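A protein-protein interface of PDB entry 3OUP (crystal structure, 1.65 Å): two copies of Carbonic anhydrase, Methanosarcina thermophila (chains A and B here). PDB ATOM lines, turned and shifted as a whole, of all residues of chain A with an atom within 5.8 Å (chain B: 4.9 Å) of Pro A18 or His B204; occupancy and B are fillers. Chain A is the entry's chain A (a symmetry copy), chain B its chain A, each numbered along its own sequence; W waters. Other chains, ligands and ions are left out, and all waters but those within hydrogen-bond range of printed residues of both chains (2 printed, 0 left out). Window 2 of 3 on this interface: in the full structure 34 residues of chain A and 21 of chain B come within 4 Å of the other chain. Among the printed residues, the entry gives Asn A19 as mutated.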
ATOM      1  N   VAL A  16      -4.799 -16.767  23.594  1.00  0.00           N
ATOM      2  CA  VAL A  16      -5.705 -17.843  23.179  1.00  0.00           C
ATOM      3  C   VAL A  16      -7.125 -17.276  23.203  1.00  0.00           C
ATOM      4  O   VAL A  16      -7.514 -16.628  24.178  1.00  0.00           O
ATOM      5  CB  VAL A  16      -5.618 -19.040  24.129  1.00  0.00           C
ATOM      6  CG1 VAL A  16      -6.651 -20.101  23.747  1.00  0.00           C
ATOM      7  CG2 VAL A  16      -4.214 -19.639  24.081  1.00  0.00           C
ATOM      8  N   THR A  17      -7.873 -17.487  22.124  1.00  0.00           N
ATOM      9  CA  THR A  17      -9.264 -17.057  22.041  1.00  0.00           C
ATOM     10  C   THR A  17     -10.050 -18.115  21.286  1.00  0.00           C
ATOM     11  O   THR A  17      -9.467 -19.048  20.737  1.00  0.00           O
ATOM     12  CB  THR A  17      -9.436 -15.736  21.248  1.00  0.00           C
ATOM     13  OG1 THR A  17      -9.121 -15.970  19.871  1.00  0.00           O
ATOM     14  CG2 THR A  17      -8.529 -14.632  21.816  1.00  0.00           C
ATOM     15  N   PRO A  18     -11.383 -17.972  21.240  1.00  0.00           N
ATOM     16  CA  PRO A  18     -12.094 -18.998  20.461  1.00  0.00           C
ATOM     17  C   PRO A  18     -11.723 -18.959  18.967  1.00  0.00           C
ATOM     18  O   PRO A  18     -11.827 -19.983  18.292  1.00  0.00           O
ATOM     19  CB  PRO A  18     -13.576 -18.684  20.709  1.00  0.00           C
ATOM     20  CG  PRO A  18     -13.620 -17.320  21.311  1.00  0.00           C
ATOM     21  CD  PRO A  18     -12.285 -17.045  21.944  1.00  0.00           C
ATOM     22  N   ASN A  19     -11.266 -17.804  18.484  1.00  0.00           N
ATOM     23  CA  ASN A  19     -10.826 -17.621  17.095  1.00  0.00           C
ATOM     24  C   ASN A  19      -9.362 -17.982  16.857  1.00  0.00           C
ATOM     25  O   ASN A  19      -8.878 -17.901  15.728  1.00  0.00           O
ATOM     26  CB  ASN A  19     -11.011 -16.155  16.688  1.00  0.00           C
ATOM     27  CG  ASN A  19     -12.419 -15.668  16.928  1.00  0.00           C
ATOM     28  OD1 ASN A  19     -13.319 -15.953  16.139  1.00  0.00           O
ATOM     29  ND2 ASN A  19     -12.621 -14.922  18.019  1.00  0.00           N
ATOM     30  N   ASN A  20      -8.664 -18.358  17.926  1.00  0.00           N
ATOM     31  CA  ASN A  20      -7.211 -18.538  17.894  1.00  0.00           C
ATOM     32  C   ASN A  20      -6.752 -19.540  18.947  1.00  0.00           C
ATOM     33  O   ASN A  20      -6.389 -19.157  20.056  1.00  0.00           O
ATOM     34  CB  ASN A  20      -6.504 -17.190  18.115  1.00  0.00           C
ATOM     35  CG  ASN A  20      -4.993 -17.279  17.924  1.00  0.00           C
ATOM     36  OD1 ASN A  20      -4.515 -17.587  16.830  1.00  0.00           O
ATOM     37  ND2 ASN A  20      -4.237 -16.997  18.982  1.00  0.00           N
ATOM     38  N   PRO A  21      -6.762 -20.832  18.597  1.00  0.00           N
ATOM     39  CA  PRO A  21      -6.428 -21.958  19.478  1.00  0.00           C
ATOM     40  C   PRO A  21      -4.963 -22.003  19.922  1.00  0.00           C
ATOM     41  O   PRO A  21      -4.658 -22.542  20.995  1.00  0.00           O
ATOM     42  CB  PRO A  21      -6.740 -23.187  18.608  1.00  0.00           C
ATOM     43  CG  PRO A  21      -7.646 -22.684  17.528  1.00  0.00           C
ATOM     44  CD  PRO A  21      -7.240 -21.282  17.278  1.00  0.00           C
ATOM     45  N   ASN A  87     -14.019 -17.287  12.098  1.00  0.00           N
ATOM     46  CA  ASN A  87     -15.062 -17.137  13.118  1.00  0.00           C
ATOM     47  C   ASN A  87     -14.955 -18.250  14.168  1.00  0.00           C
ATOM     48  O   ASN A  87     -14.081 -19.115  14.071  1.00  0.00           O
ATOM     49  CB  ASN A  87     -16.468 -17.060  12.499  1.00  0.00           C
ATOM     50  CG  ASN A  87     -16.919 -18.368  11.876  1.00  0.00           C
ATOM     51  OD1 ASN A  87     -16.384 -19.437  12.175  1.00  0.00           O
ATOM     52  ND2 ASN A  87     -17.921 -18.287  11.004  1.00  0.00           N
ATOM     53  N   GLU A  88     -15.821 -18.222  15.177  1.00  0.00           N
ATOM     54  CA  GLU A  88     -15.672 -19.128  16.313  1.00  0.00           C
ATOM     55  C   GLU A  88     -15.783 -20.586  15.901  1.00  0.00           C
ATOM     56  O   GLU A  88     -15.188 -21.461  16.523  1.00  0.00           O
ATOM     57  CB  GLU A  88     -16.707 -18.830  17.393  1.00  0.00           C
ATOM     58  CG  GLU A  88     -16.406 -17.600  18.209  1.00  0.00           C
ATOM     59  CD  GLU A  88     -17.387 -17.423  19.332  1.00  0.00           C
ATOM     60  OE1 GLU A  88     -18.504 -16.959  19.050  1.00  0.00           O
ATOM     61  OE2 GLU A  88     -17.052 -17.764  20.484  1.00  0.00           O
ATOM     62  N   TYR B 200     -18.165  -8.153  20.541  1.00  0.00           N
ATOM     63  CA  TYR B 200     -18.099  -9.568  20.877  1.00  0.00           C
ATOM     64  C   TYR B 200     -16.643 -10.034  20.883  1.00  0.00           C
ATOM     65  O   TYR B 200     -16.192 -10.715  21.835  1.00  0.00           O
ATOM     66  CB  TYR B 200     -18.895 -10.354  19.842  1.00  0.00           C
ATOM     67  CG  TYR B 200     -18.974 -11.823  20.130  1.00  0.00           C
ATOM     68  CD1 TYR B 200     -19.909 -12.319  21.042  1.00  0.00           C
ATOM     69  CD2 TYR B 200     -18.126 -12.715  19.485  1.00  0.00           C
ATOM     70  CE1 TYR B 200     -20.001 -13.688  21.300  1.00  0.00           C
ATOM     71  CE2 TYR B 200     -18.213 -14.094  19.756  1.00  0.00           C
ATOM     72  CZ  TYR B 200     -19.144 -14.553  20.660  1.00  0.00           C
ATOM     73  OH  TYR B 200     -19.256 -15.898  20.935  1.00  0.00           O
ATOM     74  N   VAL B 201     -15.924  -9.684  19.818  1.00  0.00           N
ATOM     75  CA  VAL B 201     -14.506 -10.078  19.709  1.00  0.00           C
ATOM     76  C   VAL B 201     -13.659  -9.472  20.816  1.00  0.00           C
ATOM     77  O   VAL B 201     -12.805 -10.155  21.393  1.00  0.00           O
ATOM     78  CB  VAL B 201     -13.938  -9.659  18.343  1.00  0.00           C
ATOM     79  CG1 VAL B 201     -12.425  -9.753  18.345  1.00  0.00           C
ATOM     80  CG2 VAL B 201     -14.544 -10.533  17.260  1.00  0.00           C
ATOM     81  N   ASN B 202     -13.858  -8.196  21.118  1.00  0.00           N
ATOM     82  CA  ASN B 202     -13.019  -7.536  22.125  1.00  0.00           C
ATOM     83  C   ASN B 202     -13.280  -8.016  23.536  1.00  0.00           C
ATOM     84  O   ASN B 202     -12.361  -8.011  24.354  1.00  0.00           O
ATOM     85  CB  ASN B 202     -13.148  -6.019  22.075  1.00  0.00           C
ATOM     86  CG  ASN B 202     -12.230  -5.391  21.053  1.00  0.00           C
ATOM     87  OD1 ASN B 202     -11.074  -5.069  21.359  1.00  0.00           O
ATOM     88  ND2 ASN B 202     -12.750  -5.165  19.856  1.00  0.00           N
ATOM     89  N   VAL B 203     -14.514  -8.415  23.844  1.00  0.00           N
ATOM     90  CA  VAL B 203     -14.780  -8.958  25.186  1.00  0.00           C
ATOM     91  C   VAL B 203     -13.961 -10.240  25.321  1.00  0.00           C
ATOM     92  O   VAL B 203     -13.353 -10.505  26.372  1.00  0.00           O
ATOM     93  CB  VAL B 203     -16.288  -9.185  25.390  1.00  0.00           C
ATOM     94  CG1 VAL B 203     -16.539 -10.141  26.581  1.00  0.00           C
ATOM     95  CG2 VAL B 203     -16.949  -7.813  25.640  1.00  0.00           C
ATOM     96  N   HIS B 204     -13.915 -11.049  24.260  1.00  0.00           N
ATOM     97  CA  HIS B 204     -13.096 -12.273  24.307  1.00  0.00           C
ATOM     98  C   HIS B 204     -11.607 -12.033  24.290  1.00  0.00           C
ATOM     99  O   HIS B 204     -10.835 -12.791  24.936  1.00  0.00           O
ATOM    100  CB  HIS B 204     -13.493 -13.208  23.163  1.00  0.00           C
ATOM    101  CG  HIS B 204     -14.824 -13.859  23.385  1.00  0.00           C
ATOM    102  ND1 HIS B 204     -16.017 -13.218  23.144  1.00  0.00           N
ATOM    103  CD2 HIS B 204     -15.149 -15.080  23.872  1.00  0.00           C
ATOM    104  CE1 HIS B 204     -17.020 -14.022  23.449  1.00  0.00           C
ATOM    105  NE2 HIS B 204     -16.521 -15.162  23.882  1.00  0.00           N
ATOM    106  N   LEU B 205     -11.165 -10.999  23.586  1.00  0.00           N
ATOM    107  CA  LEU B 205      -9.725 -10.642  23.616  1.00  0.00           C
ATOM    108  C   LEU B 205      -9.318 -10.186  24.995  1.00  0.00           C
ATOM    109  O   LEU B 205      -8.239 -10.553  25.477  1.00  0.00           O
ATOM    110  CB  LEU B 205      -9.403  -9.511  22.629  1.00  0.00           C
ATOM    111  CG  LEU B 205      -9.227  -9.915  21.182  1.00  0.00           C
ATOM    112  CD1 LEU B 205      -9.082  -8.622  20.329  1.00  0.00           C
ATOM    113  CD2 LEU B 205      -8.017 -10.839  21.052  1.00  0.00           C
ATOM    114  N   ALA B 206     -10.162  -9.401  25.659  1.00  0.00           N
ATOM    115  CA  ALA B 206      -9.816  -8.927  27.001  1.00  0.00           C
ATOM    116  C   ALA B 206      -9.585 -10.134  27.935  1.00  0.00           C
ATOM    117  O   ALA B 206      -8.634 -10.134  28.719  1.00  0.00           O
ATOM    118  CB  ALA B 206     -10.885  -8.027  27.542  1.00  0.00           C
ATOM    119  N   GLU B 207     -10.437 -11.153  27.838  1.00  0.00           N
ATOM    120  CA  GLU B 207     -10.294 -12.326  28.690  1.00  0.00           C
ATOM    121  C   GLU B 207      -9.012 -13.086  28.348  1.00  0.00           C
ATOM    122  O   GLU B 207      -8.313 -13.576  29.225  1.00  0.00           O
ATOM    123  CB  GLU B 207     -11.492 -13.251  28.514  1.00  0.00           C
ATOM    124  CG  GLU B 207     -11.364 -14.570  29.301  1.00  0.00           C
ATOM    125  CD  GLU B 207     -11.187 -14.380  30.811  1.00  0.00           C
ATOM    126  OE1 GLU B 207     -11.141 -13.229  31.289  1.00  0.00           O
ATOM    127  OE2 GLU B 207     -11.096 -15.399  31.527  1.00  0.00           O
ATOM    128  N   GLY B 208      -8.700 -13.187  27.059  1.00  0.00           N
ATOM    129  CA  GLY B 208      -7.502 -13.896  26.634  1.00  0.00           C
ATOM    130  C   GLY B 208      -6.237 -13.144  27.078  1.00  0.00           C
ATOM    131  O   GLY B 208      -5.269 -13.785  27.576  1.00  0.00           O
HETATM  132  O   HOH W   1     -11.513 -12.825  20.283  1.00  0.00           O
HETATM  133  O   HOH W   2     -10.578 -15.563  25.121  1.00  0.00           O
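No position is printed for both chains.
OG1 of Thr A17 lies close to N of Asn A19 (3.1 Å).
The side-chain hydroxyl (OG1) of Thr A17 sits at hydrogen-bond distance from the backbone NH (N) of Asn A20, 3.1 Å away.
The backbone carbonyl oxygen (O) of Tyr B200 is in hydrogen-bond range of a ring nitrogen (ND1) of His B204.
OH of Tyr B200 sits close to OE2 of Glu A88 (2.9 Å).
Among the printed residues, pairs that only touch across the chains: Val A16 with Gly B208 (3.7 Å), Thr A17 with Leu B205 (3.9 Å) and Pro A18 with His B204 (3.7 Å).
Of the printed residues of chain B, Pro A18 touches His B204.
His B204 touches just one residue of chain A: Pro A18.
Printed residues of chain B within 4 Å of Thr A17: Leu B205 (3.9 Å).
Printed residues of chain A within 4 Å of Tyr B200: Glu A88.
Printed residues of chain A within 4 Å of Leu B205: Thr A17.
Val B201 touches none of the printed residues of chain A.
The nearest printed residue of chain A that does not touch His B204 is Thr A17 (4.3 Å).
The nearest printed residue of chain B that does not touch Val A16 is His B204 (5.1 Å).
Of the 9 printed residues of chain B, 4 touch a printed residue of chain A.
Hydrophobic or aromatic side chains of chain B within 4 Å of the printed part of chain A: Tyr B200, His B204 and Leu B205.
Along chain B the printed residues that touch a printed residue of chain A span positions 200 to 208.
Of the 8 printed residues of chain A, 4 touch a printed residue of chain B.
Hydrophobic or aromatic side chains of chain A that line the printed part of chain B: Pro A18.
Water W2 lies within hydrogen-bond range of the backbone carbonyl oxygen (O) of His B204 (2.8 Å) and the backbone carbonyl oxygen (O) of Val A16 (3.4 Å).
Water W1 lies within hydrogen-bond range of the backbone carbonyl oxygen of Val B201 (3.2 Å) and the side-chain amide nitrogen of Asn A19 (3.3 Å).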
